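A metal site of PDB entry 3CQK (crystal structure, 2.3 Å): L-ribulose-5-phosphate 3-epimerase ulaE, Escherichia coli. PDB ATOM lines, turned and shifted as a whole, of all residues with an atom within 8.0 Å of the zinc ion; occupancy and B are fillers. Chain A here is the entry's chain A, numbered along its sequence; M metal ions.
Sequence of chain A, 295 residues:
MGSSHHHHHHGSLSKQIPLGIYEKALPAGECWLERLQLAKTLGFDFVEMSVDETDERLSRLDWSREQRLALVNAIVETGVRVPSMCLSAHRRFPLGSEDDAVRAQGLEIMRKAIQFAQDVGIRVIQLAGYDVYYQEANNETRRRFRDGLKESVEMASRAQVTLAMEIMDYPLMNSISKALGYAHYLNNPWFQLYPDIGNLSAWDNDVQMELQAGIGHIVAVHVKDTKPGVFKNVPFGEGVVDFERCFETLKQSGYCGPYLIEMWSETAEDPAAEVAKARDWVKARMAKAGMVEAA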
ATOM      1  N   TYR A  22     -20.629 -10.280   6.897  1.00  0.00           N
ATOM      2  CA  TYR A  22     -20.868 -10.622   8.306  1.00  0.00           C
ATOM      3  C   TYR A  22     -19.707 -10.145   9.184  1.00  0.00           C
ATOM      4  O   TYR A  22     -18.550 -10.220   8.777  1.00  0.00           O
ATOM      5  CB  TYR A  22     -21.029 -12.133   8.453  1.00  0.00           C
ATOM      6  CG  TYR A  22     -21.716 -12.609   9.725  1.00  0.00           C
ATOM      7  CD1 TYR A  22     -22.922 -12.065  10.145  1.00  0.00           C
ATOM      8  CD2 TYR A  22     -21.169 -13.654  10.469  1.00  0.00           C
ATOM      9  CE1 TYR A  22     -23.572 -12.503  11.300  1.00  0.00           C
ATOM     10  CE2 TYR A  22     -21.807 -14.127  11.619  1.00  0.00           C
ATOM     11  CZ  TYR A  22     -23.003 -13.543  12.032  1.00  0.00           C
ATOM     12  OH  TYR A  22     -23.639 -13.985  13.182  1.00  0.00           O
ATOM     13  N   GLU A  48     -22.835  -6.459   8.724  1.00  0.00           N
ATOM     14  CA  GLU A  48     -23.888  -6.889   9.635  1.00  0.00           C
ATOM     15  C   GLU A  48     -23.323  -7.240  11.009  1.00  0.00           C
ATOM     16  O   GLU A  48     -22.446  -8.103  11.127  1.00  0.00           O
ATOM     17  CB  GLU A  48     -24.679  -8.059   9.040  1.00  0.00           C
ATOM     18  CG  GLU A  48     -25.669  -8.713   9.984  1.00  0.00           C
ATOM     19  CD  GLU A  48     -26.637  -9.607   9.232  1.00  0.00           C
ATOM     20  OE1 GLU A  48     -26.503 -10.847   9.308  1.00  0.00           O
ATOM     21  OE2 GLU A  48     -27.510  -9.043   8.527  1.00  0.00           O
ATOM     22  N   CYS A  86     -27.773  -9.330  13.506  1.00  0.00           N
ATOM     23  CA  CYS A  86     -28.061 -10.756  13.681  1.00  0.00           C
ATOM     24  C   CYS A  86     -28.256 -10.981  15.192  1.00  0.00           C
ATOM     25  O   CYS A  86     -27.332 -10.765  15.966  1.00  0.00           O
ATOM     26  CB  CYS A  86     -26.856 -11.553  13.166  1.00  0.00           C
ATOM     27  SG  CYS A  86     -26.824 -13.370  13.423  1.00  0.00           S
ATOM     28  N   GLN A 126     -32.406  -9.202  12.475  1.00  0.00           N
ATOM     29  CA  GLN A 126     -32.660 -10.577  12.102  1.00  0.00           C
ATOM     30  C   GLN A 126     -32.926 -11.439  13.330  1.00  0.00           C
ATOM     31  O   GLN A 126     -32.058 -11.607  14.190  1.00  0.00           O
ATOM     32  CB  GLN A 126     -31.465 -11.144  11.343  1.00  0.00           C
ATOM     33  CG  GLN A 126     -31.749 -12.500  10.676  1.00  0.00           C
ATOM     34  CD  GLN A 126     -30.508 -13.089  10.013  1.00  0.00           C
ATOM     35  OE1 GLN A 126     -29.420 -13.075  10.601  1.00  0.00           O
ATOM     36  NE2 GLN A 126     -30.658 -13.605   8.770  1.00  0.00           N
ATOM     37  N   GLU A 166     -35.107 -15.018  10.170  1.00  0.00           N
ATOM     38  CA  GLU A 166     -34.230 -15.838   9.365  1.00  0.00           C
ATOM     39  C   GLU A 166     -34.840 -17.200   9.054  1.00  0.00           C
ATOM     40  O   GLU A 166     -35.535 -17.791   9.888  1.00  0.00           O
ATOM     41  CB  GLU A 166     -32.835 -16.020   9.998  1.00  0.00           C
ATOM     42  CG  GLU A 166     -31.803 -16.488   8.957  1.00  0.00           C
ATOM     43  CD  GLU A 166     -30.436 -16.830   9.510  1.00  0.00           C
ATOM     44  OE1 GLU A 166     -30.295 -16.938  10.758  1.00  0.00           O
ATOM     45  OE2 GLU A 166     -29.484 -16.983   8.688  1.00  0.00           O
ATOM     46  N   ILE A 167     -34.560 -17.699   7.860  1.00  0.00           N
ATOM     47  CA  ILE A 167     -34.812 -19.100   7.571  1.00  0.00           C
ATOM     48  C   ILE A 167     -33.611 -19.887   8.114  1.00  0.00           C
ATOM     49  O   ILE A 167     -32.437 -19.614   7.785  1.00  0.00           O
ATOM     50  CB  ILE A 167     -35.090 -19.343   6.083  1.00  0.00           C
ATOM     51  CG1 ILE A 167     -36.533 -18.955   5.739  1.00  0.00           C
ATOM     52  CG2 ILE A 167     -34.903 -20.829   5.725  1.00  0.00           C
ATOM     53  CD1 ILE A 167     -36.893 -17.478   5.894  1.00  0.00           C
ATOM     54  N   MET A 168     -33.928 -20.857   8.959  1.00  0.00           N
ATOM     55  CA  MET A 168     -33.018 -21.393   9.983  1.00  0.00           C
ATOM     56  C   MET A 168     -32.454 -22.783   9.700  1.00  0.00           C
ATOM     57  O   MET A 168     -32.961 -23.551   8.861  1.00  0.00           O
ATOM     58  CB  MET A 168     -33.763 -21.483  11.324  1.00  0.00           C
ATOM     59  CG  MET A 168     -34.384 -20.185  11.821  1.00  0.00           C
ATOM     60  SD  MET A 168     -33.114 -18.956  12.181  1.00  0.00           S
ATOM     61  CE  MET A 168     -32.186 -19.846  13.401  1.00  0.00           C
ATOM     62  N   ASP A 169     -31.414 -23.096  10.468  1.00  0.00           N
ATOM     63  CA  ASP A 169     -30.844 -24.431  10.601  1.00  0.00           C
ATOM     64  C   ASP A 169     -31.636 -25.276  11.608  1.00  0.00           C
ATOM     65  O   ASP A 169     -31.072 -26.059  12.362  1.00  0.00           O
ATOM     66  CB  ASP A 169     -29.379 -24.329  11.067  1.00  0.00           C
ATOM     67  CG  ASP A 169     -29.220 -23.761  12.486  1.00  0.00           C
ATOM     68  OD1 ASP A 169     -30.108 -22.999  12.965  1.00  0.00           O
ATOM     69  OD2 ASP A 169     -28.196 -24.091  13.142  1.00  0.00           O
ATOM     70  N   TYR A 194     -36.062 -12.717   6.255  1.00  0.00           N
ATOM     71  CA  TYR A 194     -34.657 -12.592   5.971  1.00  0.00           C
ATOM     72  C   TYR A 194     -34.158 -14.005   5.651  1.00  0.00           C
ATOM     73  O   TYR A 194     -33.562 -14.667   6.512  1.00  0.00           O
ATOM     74  CB  TYR A 194     -33.938 -12.024   7.203  1.00  0.00           C
ATOM     75  CG  TYR A 194     -32.531 -11.490   6.987  1.00  0.00           C
ATOM     76  CD1 TYR A 194     -32.047 -10.457   7.780  1.00  0.00           C
ATOM     77  CD2 TYR A 194     -31.683 -12.035   6.028  1.00  0.00           C
ATOM     78  CE1 TYR A 194     -30.748  -9.966   7.606  1.00  0.00           C
ATOM     79  CE2 TYR A 194     -30.399 -11.546   5.834  1.00  0.00           C
ATOM     80  CZ  TYR A 194     -29.933 -10.508   6.640  1.00  0.00           C
ATOM     81  OH  TYR A 194     -28.651 -10.023   6.469  1.00  0.00           O
ATOM     82  N   PRO A 195     -34.401 -14.489   4.422  1.00  0.00           N
ATOM     83  CA  PRO A 195     -33.981 -15.868   4.136  1.00  0.00           C
ATOM     84  C   PRO A 195     -32.479 -16.039   4.045  1.00  0.00           C
ATOM     85  O   PRO A 195     -31.763 -15.137   3.616  1.00  0.00           O
ATOM     86  CB  PRO A 195     -34.612 -16.162   2.760  1.00  0.00           C
ATOM     87  CG  PRO A 195     -34.810 -14.813   2.136  1.00  0.00           C
ATOM     88  CD  PRO A 195     -35.086 -13.873   3.270  1.00  0.00           C
ATOM     89  N   ASP A 196     -32.013 -17.203   4.470  1.00  0.00           N
ATOM     90  CA  ASP A 196     -30.653 -17.610   4.238  1.00  0.00           C
ATOM     91  C   ASP A 196     -30.736 -18.687   3.157  1.00  0.00           C
ATOM     92  O   ASP A 196     -31.320 -19.740   3.368  1.00  0.00           O
ATOM     93  CB  ASP A 196     -30.050 -18.148   5.547  1.00  0.00           C
ATOM     94  CG  ASP A 196     -28.630 -18.633   5.387  1.00  0.00           C
ATOM     95  OD1 ASP A 196     -28.330 -19.449   4.481  1.00  0.00           O
ATOM     96  OD2 ASP A 196     -27.797 -18.208   6.205  1.00  0.00           O
ATOM     97  N   ILE A 197     -30.142 -18.422   2.000  1.00  0.00           N
ATOM     98  CA  ILE A 197     -30.318 -19.352   0.895  1.00  0.00           C
ATOM     99  C   ILE A 197     -29.570 -20.685   1.130  1.00  0.00           C
ATOM    100  O   ILE A 197     -29.836 -21.677   0.448  1.00  0.00           O
ATOM    101  CB  ILE A 197     -29.944 -18.723  -0.470  1.00  0.00           C
ATOM    102  CG1 ILE A 197     -28.467 -18.359  -0.537  1.00  0.00           C
ATOM    103  CG2 ILE A 197     -30.897 -17.524  -0.805  1.00  0.00           C
ATOM    104  CD1 ILE A 197     -28.022 -17.903  -1.924  1.00  0.00           C
ATOM    105  N   GLY A 198     -28.663 -20.685   2.122  1.00  0.00           N
ATOM    106  CA  GLY A 198     -27.952 -21.889   2.503  1.00  0.00           C
ATOM    107  C   GLY A 198     -28.799 -22.777   3.376  1.00  0.00           C
ATOM    108  O   GLY A 198     -28.983 -23.945   3.094  1.00  0.00           O
ATOM    109  N   ASN A 199     -29.311 -22.194   4.457  1.00  0.00           N
ATOM    110  CA  ASN A 199     -30.239 -22.880   5.334  1.00  0.00           C
ATOM    111  C   ASN A 199     -31.450 -23.401   4.568  1.00  0.00           C
ATOM    112  O   ASN A 199     -31.893 -24.534   4.816  1.00  0.00           O
ATOM    113  CB  ASN A 199     -30.684 -21.937   6.440  1.00  0.00           C
ATOM    114  CG  ASN A 199     -29.609 -21.661   7.472  1.00  0.00           C
ATOM    115  OD1 ASN A 199     -28.569 -22.335   7.527  1.00  0.00           O
ATOM    116  ND2 ASN A 199     -29.863 -20.654   8.305  1.00  0.00           N
ATOM    117  N   VAL A 221     -31.052 -10.895   2.255  1.00  0.00           N
ATOM    118  CA  VAL A 221     -30.695 -12.279   1.945  1.00  0.00           C
ATOM    119  C   VAL A 221     -29.303 -12.579   2.511  1.00  0.00           C
ATOM    120  O   VAL A 221     -28.346 -11.809   2.270  1.00  0.00           O
ATOM    121  CB  VAL A 221     -30.685 -12.523   0.415  1.00  0.00           C
ATOM    122  CG1 VAL A 221     -30.365 -14.009   0.087  1.00  0.00           C
ATOM    123  CG2 VAL A 221     -32.000 -12.077  -0.228  1.00  0.00           C
ATOM    124  N   HIS A 222     -29.206 -13.677   3.275  1.00  0.00           N
ATOM    125  CA  HIS A 222     -27.936 -14.280   3.677  1.00  0.00           C
ATOM    126  C   HIS A 222     -27.374 -15.190   2.568  1.00  0.00           C
ATOM    127  O   HIS A 222     -28.072 -15.987   1.990  1.00  0.00           O
ATOM    128  CB  HIS A 222     -28.114 -15.079   4.976  1.00  0.00           C
ATOM    129  CG  HIS A 222     -27.798 -14.299   6.213  1.00  0.00           C
ATOM    130  ND1 HIS A 222     -27.530 -14.911   7.414  1.00  0.00           N
ATOM    131  CD2 HIS A 222     -27.667 -12.972   6.436  1.00  0.00           C
ATOM    132  CE1 HIS A 222     -27.290 -13.994   8.337  1.00  0.00           C
ATOM    133  NE2 HIS A 222     -27.357 -12.810   7.760  1.00  0.00           N
ATOM    134  N   VAL A 223     -26.085 -15.031   2.274  1.00  0.00           N
ATOM    135  CA  VAL A 223     -25.440 -15.843   1.232  1.00  0.00           C
ATOM    136  C   VAL A 223     -24.337 -16.705   1.860  1.00  0.00           C
ATOM    137  O   VAL A 223     -23.321 -16.181   2.342  1.00  0.00           O
ATOM    138  CB  VAL A 223     -24.919 -14.945   0.068  1.00  0.00           C
ATOM    139  CG1 VAL A 223     -24.154 -15.769  -0.974  1.00  0.00           C
ATOM    140  CG2 VAL A 223     -26.116 -14.171  -0.599  1.00  0.00           C
ATOM    141  N   LYS A 224     -24.590 -18.012   1.901  1.00  0.00           N
ATOM    142  CA  LYS A 224     -23.629 -19.028   2.349  1.00  0.00           C
ATOM    143  C   LYS A 224     -23.926 -20.411   1.745  1.00  0.00           C
ATOM    144  O   LYS A 224     -25.033 -20.659   1.236  1.00  0.00           O
ATOM    145  CB  LYS A 224     -23.561 -19.135   3.868  1.00  0.00           C
ATOM    146  CG  LYS A 224     -24.767 -19.771   4.492  1.00  0.00           C
ATOM    147  CD  LYS A 224     -24.537 -20.102   5.961  1.00  0.00           C
ATOM    148  CE  LYS A 224     -25.740 -20.909   6.443  1.00  0.00           C
ATOM    149  NZ  LYS A 224     -26.185 -20.564   7.813  1.00  0.00           N
ATOM    150  N   PHE A 231     -24.626 -26.563   8.381  1.00  0.00           N
ATOM    151  CA  PHE A 231     -25.086 -25.197   8.149  1.00  0.00           C
ATOM    152  C   PHE A 231     -24.008 -24.131   8.428  1.00  0.00           C
ATOM    153  O   PHE A 231     -24.265 -22.920   8.283  1.00  0.00           O
ATOM    154  CB  PHE A 231     -26.312 -24.920   9.028  1.00  0.00           C
ATOM    155  CG  PHE A 231     -27.413 -25.921   8.861  1.00  0.00           C
ATOM    156  CD1 PHE A 231     -28.404 -25.735   7.906  1.00  0.00           C
ATOM    157  CD2 PHE A 231     -27.473 -27.037   9.685  1.00  0.00           C
ATOM    158  CE1 PHE A 231     -29.441 -26.655   7.760  1.00  0.00           C
ATOM    159  CE2 PHE A 231     -28.503 -27.961   9.544  1.00  0.00           C
ATOM    160  CZ  PHE A 231     -29.497 -27.771   8.576  1.00  0.00           C
ATOM    161  N   LEU A 260     -25.944 -10.287   1.964  1.00  0.00           N
ATOM    162  CA  LEU A 260     -24.901 -10.354   2.990  1.00  0.00           C
ATOM    163  C   LEU A 260     -24.165 -11.697   2.941  1.00  0.00           C
ATOM    164  O   LEU A 260     -24.759 -12.749   3.170  1.00  0.00           O
ATOM    165  CB  LEU A 260     -25.520 -10.129   4.368  1.00  0.00           C
ATOM    166  CG  LEU A 260     -24.810 -10.070   5.741  1.00  0.00           C
ATOM    167  CD1 LEU A 260     -24.316 -11.436   6.212  1.00  0.00           C
ATOM    168  CD2 LEU A 260     -23.714  -9.070   5.744  1.00  0.00           C
ATOM    169  N   ILE A 261     -22.866 -11.649   2.646  1.00  0.00           N
ATOM    170  CA  ILE A 261     -21.991 -12.803   2.704  1.00  0.00           C
ATOM    171  C   ILE A 261     -21.731 -13.225   4.136  1.00  0.00           C
ATOM    172  O   ILE A 261     -21.166 -12.483   4.940  1.00  0.00           O
ATOM    173  CB  ILE A 261     -20.643 -12.522   2.024  1.00  0.00           C
ATOM    174  CG1 ILE A 261     -20.841 -12.181   0.550  1.00  0.00           C
ATOM    175  CG2 ILE A 261     -19.684 -13.746   2.180  1.00  0.00           C
ATOM    176  CD1 ILE A 261     -19.539 -11.846  -0.158  1.00  0.00           C
ATOM    177  N   GLU A 262     -22.177 -14.434   4.455  1.00  0.00           N
ATOM    178  CA  GLU A 262     -22.045 -14.976   5.796  1.00  0.00           C
ATOM    179  C   GLU A 262     -20.938 -16.033   5.857  1.00  0.00           C
ATOM    180  O   GLU A 262     -21.045 -17.100   5.269  1.00  0.00           O
ATOM    181  CB  GLU A 262     -23.383 -15.545   6.249  1.00  0.00           C
ATOM    182  CG  GLU A 262     -23.294 -16.322   7.539  1.00  0.00           C
ATOM    183  CD  GLU A 262     -24.640 -16.567   8.137  1.00  0.00           C
ATOM    184  OE1 GLU A 262     -25.610 -16.802   7.383  1.00  0.00           O
ATOM    185  OE2 GLU A 262     -24.731 -16.526   9.387  1.00  0.00           O
ATOM    186  N   MET A 263     -19.882 -15.709   6.599  1.00  0.00           N
ATOM    187  CA  MET A 263     -18.778 -16.627   6.861  1.00  0.00           C
ATOM    188  C   MET A 263     -18.140 -16.276   8.205  1.00  0.00           C
ATOM    189  O   MET A 263     -18.455 -15.239   8.806  1.00  0.00           O
ATOM    190  CB  MET A 263     -17.749 -16.549   5.730  1.00  0.00           C
ATOM    191  CG  MET A 263     -17.332 -15.132   5.456  1.00  0.00           C
ATOM    192  SD  MET A 263     -16.553 -14.962   3.889  1.00  0.00           S
ATOM    193  CE  MET A 263     -15.078 -16.004   4.080  1.00  0.00           C
ATOM    194  N   TRP A 264     -17.243 -17.142   8.670  1.00  0.00           N
ATOM    195  CA  TRP A 264     -16.692 -17.052  10.019  1.00  0.00           C
ATOM    196  C   TRP A 264     -15.164 -17.025  10.040  1.00  0.00           C
ATOM    197  O   TRP A 264     -14.525 -17.598  10.922  1.00  0.00           O
ATOM    198  CB  TRP A 264     -17.216 -18.201  10.902  1.00  0.00           C
ATOM    199  CG  TRP A 264     -18.682 -18.135  11.144  1.00  0.00           C
ATOM    200  CD1 TRP A 264     -19.304 -17.601  12.244  1.00  0.00           C
ATOM    201  CD2 TRP A 264     -19.729 -18.601  10.273  1.00  0.00           C
ATOM    202  NE1 TRP A 264     -20.673 -17.721  12.111  1.00  0.00           N
ATOM    203  CE2 TRP A 264     -20.961 -18.335  10.919  1.00  0.00           C
ATOM    204  CE3 TRP A 264     -19.743 -19.241   9.020  1.00  0.00           C
ATOM    205  CZ2 TRP A 264     -22.206 -18.674  10.357  1.00  0.00           C
ATOM    206  CZ3 TRP A 264     -20.975 -19.584   8.454  1.00  0.00           C
ATOM    207  CH2 TRP A 264     -22.191 -19.297   9.131  1.00  0.00           C
HETATM  208 ZN    ZN M   1     -27.595 -16.906   7.841  1.00  0.00          ZN
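The side-chain hydroxyl (OH) of Tyr 194 sits close to a ring nitrogen (NE2) of His 222 (3.3 Å). N of Glu 262 sits at hydrogen-bond distance from O of Val 223, 3.0 Å away. A ring nitrogen (NE2) of His 222 sits at hydrogen-bond distance from the side-chain carboxylate (OE1) of Glu 48. The side-chain carboxylate (OE1) of Glu 262 lies close to the side-chain amino group (NZ) of Lys 224 (3.8 Å). The side-chain carboxylate (OD1) of Asp 196 is in hydrogen-bond range of the backbone NH (N) of Asn 199 (2.9 Å). The side-chain amino group of Lys 224 sits close to the side-chain carboxylate of Asp 196. O of Phe 231 lies within hydrogen-bond range of NZ of Lys 224 (3.1 Å). The backbone carbonyl oxygen of His 222 sits at hydrogen-bond distance from the backbone NH of Ile 197 (3.2 Å).
NZ of Lys 224 touches the zinc ion, 3.9 Å away.
OE1 of Glu 262 is bound to the zinc ion (2.0 Å). A ring nitrogen (ND1) of His 222 binds the zinc ion, at 2.0 Å. The zinc ion is bound by OE2 of Glu 166. The zinc ion is bound by OD2 of Asp 196, 2.1 Å away. The zinc ion has four donor atoms within binding distance.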
